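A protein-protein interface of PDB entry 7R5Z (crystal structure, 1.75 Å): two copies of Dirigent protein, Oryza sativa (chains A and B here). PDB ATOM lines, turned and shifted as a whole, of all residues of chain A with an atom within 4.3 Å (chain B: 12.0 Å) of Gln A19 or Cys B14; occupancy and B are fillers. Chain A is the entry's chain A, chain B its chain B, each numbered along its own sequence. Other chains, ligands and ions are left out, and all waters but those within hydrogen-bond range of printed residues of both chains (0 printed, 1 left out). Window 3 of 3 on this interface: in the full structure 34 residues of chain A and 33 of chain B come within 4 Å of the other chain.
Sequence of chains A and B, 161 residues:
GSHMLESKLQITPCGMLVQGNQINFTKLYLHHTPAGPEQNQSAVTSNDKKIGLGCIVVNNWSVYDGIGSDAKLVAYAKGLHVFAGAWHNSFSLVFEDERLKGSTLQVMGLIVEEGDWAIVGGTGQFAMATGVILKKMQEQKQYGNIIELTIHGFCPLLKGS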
ATOM      1  N   LEU A  17     -13.174  12.218 -21.834  1.00  0.00           N
ATOM      2  CA  LEU A  17     -13.599  13.372 -22.617  1.00  0.00           C
ATOM      3  C   LEU A  17     -13.999  12.987 -24.042  1.00  0.00           C
ATOM      4  O   LEU A  17     -13.505  12.005 -24.602  1.00  0.00           O
ATOM      5  CB  LEU A  17     -12.485  14.420 -22.665  1.00  0.00           C
ATOM      6  N   VAL A  18     -14.902  13.788 -24.623  1.00  0.00           N
ATOM      7  CA  VAL A  18     -15.362  13.616 -26.002  1.00  0.00           C
ATOM      8  C   VAL A  18     -14.891  14.822 -26.823  1.00  0.00           C
ATOM      9  O   VAL A  18     -15.361  15.946 -26.617  1.00  0.00           O
ATOM     10  CB  VAL A  18     -16.890  13.468 -26.091  1.00  0.00           C
ATOM     11  CG1 VAL A  18     -17.278  12.901 -27.441  1.00  0.00           C
ATOM     12  CG2 VAL A  18     -17.434  12.615 -24.950  1.00  0.00           C
ATOM     13  N   GLN A  19     -13.978  14.573 -27.768  1.00  0.00           N
ATOM     14  CA  GLN A  19     -13.482  15.614 -28.655  1.00  0.00           C
ATOM     15  C   GLN A  19     -14.604  16.133 -29.540  1.00  0.00           C
ATOM     16  O   GLN A  19     -15.395  15.364 -30.092  1.00  0.00           O
ATOM     17  CB  GLN A  19     -12.343  15.085 -29.529  1.00  0.00           C
ATOM     18  CG  GLN A  19     -11.364  14.168 -28.809  1.00  0.00           C
ATOM     19  CD  GLN A  19     -10.428  14.915 -27.879  1.00  0.00           C
ATOM     20  OE1 GLN A  19     -10.824  15.874 -27.211  1.00  0.00           O
ATOM     21  NE2 GLN A  19      -9.169  14.480 -27.834  1.00  0.00           N
ATOM     22  N   GLY A  20     -14.676  17.448 -29.672  1.00  0.00           N
ATOM     23  CA  GLY A  20     -15.710  18.018 -30.500  1.00  0.00           C
ATOM     24  C   GLY A  20     -15.440  19.473 -30.799  1.00  0.00           C
ATOM     25  O   GLY A  20     -14.332  19.981 -30.597  1.00  0.00           O
ATOM     26  N   GLN A  22     -17.228  23.358 -30.314  1.00  0.00           N
ATOM     27  CA  GLN A  22     -18.257  24.233 -29.779  1.00  0.00           C
ATOM     28  C   GLN A  22     -18.793  25.095 -30.911  1.00  0.00           C
ATOM     29  O   GLN A  22     -18.045  25.557 -31.768  1.00  0.00           O
ATOM     30  CB  GLN A  22     -17.680  25.085 -28.654  1.00  0.00           C
ATOM     31  CG  GLN A  22     -18.700  25.712 -27.750  1.00  0.00           C
ATOM     32  CD  GLN A  22     -18.050  26.568 -26.689  1.00  0.00           C
ATOM     33  OE1 GLN A  22     -17.049  26.170 -26.084  1.00  0.00           O
ATOM     34  NE2 GLN A  22     -18.595  27.760 -26.473  1.00  0.00           N
ATOM     35  N   PHE A 154     -22.635  22.311 -29.029  1.00  0.00           N
ATOM     36  CA  PHE A 154     -21.437  21.484 -29.083  1.00  0.00           C
ATOM     37  C   PHE A 154     -21.752  20.272 -29.937  1.00  0.00           C
ATOM     38  O   PHE A 154     -22.792  19.645 -29.741  1.00  0.00           O
ATOM     39  CB  PHE A 154     -21.012  21.049 -27.678  1.00  0.00           C
ATOM     40  CG  PHE A 154     -19.882  20.051 -27.662  1.00  0.00           C
ATOM     41  CD1 PHE A 154     -18.564  20.472 -27.662  1.00  0.00           C
ATOM     42  CD2 PHE A 154     -20.143  18.685 -27.637  1.00  0.00           C
ATOM     43  CE1 PHE A 154     -17.530  19.551 -27.640  1.00  0.00           C
ATOM     44  CE2 PHE A 154     -19.108  17.761 -27.618  1.00  0.00           C
ATOM     45  CZ  PHE A 154     -17.797  18.200 -27.624  1.00  0.00           C
ATOM     46  N   PRO A 156     -20.019  16.605 -30.915  1.00  0.00           N
ATOM     47  CA  PRO A 156     -18.904  15.664 -30.791  1.00  0.00           C
ATOM     48  C   PRO A 156     -18.416  15.205 -32.156  1.00  0.00           C
ATOM     49  O   PRO A 156     -19.177  15.133 -33.123  1.00  0.00           O
ATOM     50  CB  PRO A 156     -19.511  14.498 -30.003  1.00  0.00           C
ATOM     51  CG  PRO A 156     -20.963  14.544 -30.337  1.00  0.00           C
ATOM     52  CD  PRO A 156     -21.307  16.004 -30.519  1.00  0.00           C
ATOM     53  N   LEU A 157     -17.127  14.889 -32.226  1.00  0.00           N
ATOM     54  CA  LEU A 157     -16.558  14.363 -33.461  1.00  0.00           C
ATOM     55  C   LEU A 157     -16.699  12.847 -33.518  1.00  0.00           C
ATOM     56  O   LEU A 157     -16.427  12.152 -32.536  1.00  0.00           O
ATOM     57  CB  LEU A 157     -15.090  14.766 -33.594  1.00  0.00           C
ATOM     58  CG  LEU A 157     -14.870  16.257 -33.858  1.00  0.00           C
ATOM     59  CD1 LEU A 157     -13.393  16.556 -34.082  1.00  0.00           C
ATOM     60  CD2 LEU A 157     -15.713  16.712 -35.045  1.00  0.00           C
ATOM     61  N   GLN B  10     -19.287  30.326 -35.686  1.00  0.00           N
ATOM     62  CA  GLN B  10     -17.976  30.102 -35.086  1.00  0.00           C
ATOM     63  C   GLN B  10     -17.881  28.656 -34.622  1.00  0.00           C
ATOM     64  O   GLN B  10     -18.635  28.232 -33.743  1.00  0.00           O
ATOM     65  CB  GLN B  10     -17.730  31.056 -33.917  1.00  0.00           C
ATOM     66  CG  GLN B  10     -16.386  30.892 -33.261  1.00  0.00           C
ATOM     67  CD  GLN B  10     -15.238  31.141 -34.228  1.00  0.00           C
ATOM     68  OE1 GLN B  10     -15.187  32.182 -34.899  1.00  0.00           O
ATOM     69  NE2 GLN B  10     -14.313  30.182 -34.311  1.00  0.00           N
ATOM     70  N   ILE B  11     -16.940  27.916 -35.196  1.00  0.00           N
ATOM     71  CA  ILE B  11     -16.709  26.512 -34.880  1.00  0.00           C
ATOM     72  C   ILE B  11     -15.377  26.425 -34.146  1.00  0.00           C
ATOM     73  O   ILE B  11     -14.320  26.672 -34.741  1.00  0.00           O
ATOM     74  CB  ILE B  11     -16.710  25.648 -36.148  1.00  0.00           C
ATOM     75  CG1 ILE B  11     -18.025  25.838 -36.913  1.00  0.00           C
ATOM     76  CG2 ILE B  11     -16.503  24.181 -35.796  1.00  0.00           C
ATOM     77  CD1 ILE B  11     -18.079  25.117 -38.244  1.00  0.00           C
ATOM     78  N   THR B  12     -15.418  26.100 -32.856  1.00  0.00           N
ATOM     79  CA  THR B  12     -14.234  26.134 -32.011  1.00  0.00           C
ATOM     80  C   THR B  12     -13.964  24.766 -31.394  1.00  0.00           C
ATOM     81  O   THR B  12     -14.852  24.203 -30.738  1.00  0.00           O
ATOM     82  CB  THR B  12     -14.393  27.177 -30.890  1.00  0.00           C
ATOM     83  OG1 THR B  12     -14.771  28.443 -31.452  1.00  0.00           O
ATOM     84  CG2 THR B  12     -13.090  27.327 -30.115  1.00  0.00           C
ATOM     85  N   PRO B  13     -12.761  24.208 -31.562  1.00  0.00           N
ATOM     86  CA  PRO B  13     -12.446  22.926 -30.918  1.00  0.00           C
ATOM     87  C   PRO B  13     -12.586  23.026 -29.408  1.00  0.00           C
ATOM     88  O   PRO B  13     -12.223  24.030 -28.790  1.00  0.00           O
ATOM     89  CB  PRO B  13     -10.989  22.661 -31.328  1.00  0.00           C
ATOM     90  CG  PRO B  13     -10.767  23.502 -32.535  1.00  0.00           C
ATOM     91  CD  PRO B  13     -11.637  24.714 -32.363  1.00  0.00           C
ATOM     92  N   CYS B  14     -13.090  21.953 -28.816  1.00  0.00           N
ATOM     93  CA  CYS B  14     -13.548  21.977 -27.441  1.00  0.00           C
ATOM     94  C   CYS B  14     -13.627  20.534 -26.963  1.00  0.00           C
ATOM     95  O   CYS B  14     -13.725  19.606 -27.769  1.00  0.00           O
ATOM     96  CB  CYS B  14     -14.909  22.690 -27.355  1.00  0.00           C
ATOM     97  SG  CYS B  14     -15.747  22.668 -25.776  1.00  0.00           S
ATOM     98  N   GLY B  15     -13.552  20.347 -25.650  1.00  0.00           N
ATOM     99  CA  GLY B  15     -13.759  19.049 -25.034  1.00  0.00           C
ATOM    100  C   GLY B  15     -15.033  19.070 -24.211  1.00  0.00           C
ATOM    101  O   GLY B  15     -15.436  20.119 -23.702  1.00  0.00           O
ATOM    102  N   MET B  16     -15.678  17.907 -24.094  1.00  0.00           N
ATOM    103  CA  MET B  16     -16.895  17.772 -23.300  1.00  0.00           C
ATOM    104  C   MET B  16     -16.808  16.507 -22.461  1.00  0.00           C
ATOM    105  O   MET B  16     -16.537  15.426 -22.992  1.00  0.00           O
ATOM    106  CB  MET B  16     -18.152  17.725 -24.186  1.00  0.00           C
ATOM    107  CG  MET B  16     -19.452  17.570 -23.404  1.00  0.00           C
ATOM    108  SD  MET B  16     -20.978  17.444 -24.392  1.00  0.00           S
ATOM    109  CE  MET B  16     -20.750  15.830 -25.135  1.00  0.00           C
ATOM    110  N   LEU B  17     -17.031  16.645 -21.157  1.00  0.00           N
ATOM    111  CA  LEU B  17     -17.157  15.512 -20.249  1.00  0.00           C
ATOM    112  C   LEU B  17     -18.631  15.352 -19.904  1.00  0.00           C
ATOM    113  O   LEU B  17     -19.237  16.266 -19.337  1.00  0.00           O
ATOM    114  CB  LEU B  17     -16.318  15.715 -18.987  1.00  0.00           C
ATOM    115  N   VAL B  18     -19.203  14.193 -20.249  1.00  0.00           N
ATOM    116  CA  VAL B  18     -20.647  14.000 -20.125  1.00  0.00           C
ATOM    117  C   VAL B  18     -21.077  14.039 -18.662  1.00  0.00           C
ATOM    118  O   VAL B  18     -22.055  14.705 -18.305  1.00  0.00           O
ATOM    119  CB  VAL B  18     -21.074  12.686 -20.804  1.00  0.00           C
ATOM    120  N   GLN B  19     -20.360  13.323 -17.795  1.00  0.00           N
ATOM    121  CA  GLN B  19     -20.649  13.333 -16.360  1.00  0.00           C
ATOM    122  C   GLN B  19     -20.112  14.577 -15.667  1.00  0.00           C
ATOM    123  O   GLN B  19     -19.658  14.511 -14.521  1.00  0.00           O
ATOM    124  CB  GLN B  19     -20.085  12.066 -15.717  1.00  0.00           C
ATOM    125  N   MET B 128     -28.059  21.552 -22.133  1.00  0.00           N
ATOM    126  CA  MET B 128     -27.427  20.328 -22.616  1.00  0.00           C
ATOM    127  C   MET B 128     -27.740  19.108 -21.752  1.00  0.00           C
ATOM    128  O   MET B 128     -27.026  18.105 -21.830  1.00  0.00           O
ATOM    129  CB  MET B 128     -25.909  20.509 -22.754  1.00  0.00           C
ATOM    130  CG  MET B 128     -25.518  21.595 -23.763  1.00  0.00           C
ATOM    131  SD  MET B 128     -23.726  21.789 -23.893  1.00  0.00           S
ATOM    132  CE  MET B 128     -23.370  22.557 -22.316  1.00  0.00           C
ATOM    133  N   PRO B 156     -23.353  18.223 -19.175  1.00  0.00           N
ATOM    134  CA  PRO B 156     -21.914  18.179 -19.423  1.00  0.00           C
ATOM    135  C   PRO B 156     -21.282  19.557 -19.310  1.00  0.00           C
ATOM    136  O   PRO B 156     -21.893  20.582 -19.616  1.00  0.00           O
ATOM    137  CB  PRO B 156     -21.828  17.645 -20.854  1.00  0.00           C
ATOM    138  CG  PRO B 156     -23.075  18.141 -21.496  1.00  0.00           C
ATOM    139  CD  PRO B 156     -24.132  18.074 -20.417  1.00  0.00           C
ATOM    140  N   LEU B 157     -20.041  19.566 -18.847  1.00  0.00           N
ATOM    141  CA  LEU B 157     -19.226  20.768 -18.838  1.00  0.00           C
ATOM    142  C   LEU B 157     -18.275  20.726 -20.026  1.00  0.00           C
ATOM    143  O   LEU B 157     -17.741  19.666 -20.369  1.00  0.00           O
ATOM    144  CB  LEU B 157     -18.442  20.893 -17.529  1.00  0.00           C
ATOM    145  N   LEU B 158     -18.084  21.874 -20.666  1.00  0.00           N
ATOM    146  CA  LEU B 158     -17.183  21.985 -21.800  1.00  0.00           C
ATOM    147  C   LEU B 158     -15.814  22.453 -21.320  1.00  0.00           C
ATOM    148  O   LEU B 158     -15.705  23.190 -20.337  1.00  0.00           O
ATOM    149  CB  LEU B 158     -17.739  22.951 -22.850  1.00  0.00           C
ATOM    150  CG  LEU B 158     -19.113  22.598 -23.436  1.00  0.00           C
ATOM    151  CD1 LEU B 158     -19.470  23.514 -24.601  1.00  0.00           C
ATOM    152  CD2 LEU B 158     -19.169  21.147 -23.872  1.00  0.00           C
ATOM    153  N   LYS B 159     -14.766  22.005 -22.014  1.00  0.00           N
ATOM    154  CA  LYS B 159     -13.392  22.365 -21.666  1.00  0.00           C
ATOM    155  C   LYS B 159     -12.562  22.507 -22.937  1.00  0.00           C
ATOM    156  O   LYS B 159     -13.068  22.396 -24.058  1.00  0.00           O
ATOM    157  CB  LYS B 159     -12.776  21.327 -20.721  1.00  0.00           C
ATOM    158  N   GLY B 160     -11.267  22.744 -22.761  1.00  0.00           N
ATOM    159  CA  GLY B 160     -10.375  22.878 -23.896  1.00  0.00           C
ATOM    160  C   GLY B 160     -10.309  24.285 -24.454  1.00  0.00           C
ATOM    161  O   GLY B 160     -10.357  25.262 -23.698  1.00  0.00           O
ATOM    162  N   SER B 161     -10.187  24.395 -25.776  1.00  0.00           N
ATOM    163  CA  SER B 161     -10.080  25.681 -26.470  1.00  0.00           C
ATOM    164  C   SER B 161      -8.882  26.513 -25.980  1.00  0.00           C
ATOM    165  O   SER B 161      -8.788  27.717 -26.214  1.00  0.00           O
ATOM    166  CB  SER B 161     -11.384  26.475 -26.321  1.00  0.00           C
ATOM    167  OXT SER B 161      -7.957  26.012 -25.337  1.00  0.00           O
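Of the 17 printed residues of chain B, 8 touch a printed residue of chain A.
Hydrophobic or aromatic side chains of chain B within 4 Å of the printed part of chain A: Met B16 and Leu B158.
Hydrophobic or aromatic side chains of chain A within 4 Å of the printed part of chain B: Val A18 and Phe A154.
Among the printed residues, no Asp or Glu carboxylate lies within 4 Å of a Lys or Arg side-chain nitrogen of the other chain.
Positions printed for both chains: 17, 18, 19, 156 and 157.
The backbone NH of Val A18 is in hydrogen-bond range of the backbone carbonyl oxygen of Met B16, at 2.8 Å.
SG of Cys B14 sits at hydrogen-bond distance from OE1 of Gln A22 (3.7 Å).
O of Gln B10 lies close to O of Gln A22 (3.4 Å).
The backbone NH (N) of Gln A22 is in hydrogen-bond range of the backbone carbonyl oxygen (O) of Thr B12 (2.6 Å).
N of Cys B14 lies within hydrogen-bond range of O of Gly A20, 2.9 Å away.
Printed residues of chain B within 4 Å of Gln A19: Cys B14 (3.996 Å).
Leu A17 touches just one residue of chain B: Met B16 (3.6 Å).
Of chain B, only Gly B15 and Met B16 come within 4 Å of Val A18.
Gly A20 touches just these residues of chain B: Pro B13 and Cys B14.
Gln A22 touches just these residues of chain B: Gln B10 (3.4 Å), Ile B11 (3.5 Å), Thr B12 (2.6 Å), Cys B14 (3.7 Å) and Leu B158 (3.9 Å).
No residue of chain B comes within 4 Å of Pro A156.
No residue of chain B comes within 4 Å of Leu A157.
Of the printed residues of chain A, Thr B12 touches Gln A22.
Printed residues of chain A within 4 Å of Met B16: Leu A17, Val A18 and Phe A154.
Of the printed residues of chain A, Gln B10 touches Gln A22 (3.4 Å).
Printed residues of chain A within 4 Å of Leu B158: Gln A22 and Phe A154.
Printed residues of chain A within 4 Å of Pro B13: Gly A20.
The nearest printed residue of chain A that does not touch Gln B10 is Phe A154 (8.6 Å).
NE2 of Gln B10 lies within hydrogen-bond range of OG1 of Thr B12 (3.4 Å).
The backbone carbonyl oxygen (O) of Gly B15 sits at hydrogen-bond distance from the backbone NH (N) of Lys B159 (2.6 Å).
The side-chain sulfur (SG) of Cys B14 is in hydrogen-bond range of the backbone carbonyl oxygen (O) of Lys B159, 3.2 Å away.
The backbone carbonyl oxygen (O) of Gln A19 is in hydrogen-bond range of the backbone NH (N) of Leu A157 (2.8 Å).
Met B16 touches Leu A17.
Val A18 touches Gly B15.
Gln A19 touches Cys B14.
Gly A20 touches Pro B13.
Ile B11 touches Gln A22.
Gln A22 touches Leu B158 (OE1 to CD1, 3.9 Å).
Cys B14 touches Phe A154.
Phe A154 touches Met B16.
CD2 of Leu B158 touches CD1 of Phe A154, 3.9 Å away.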
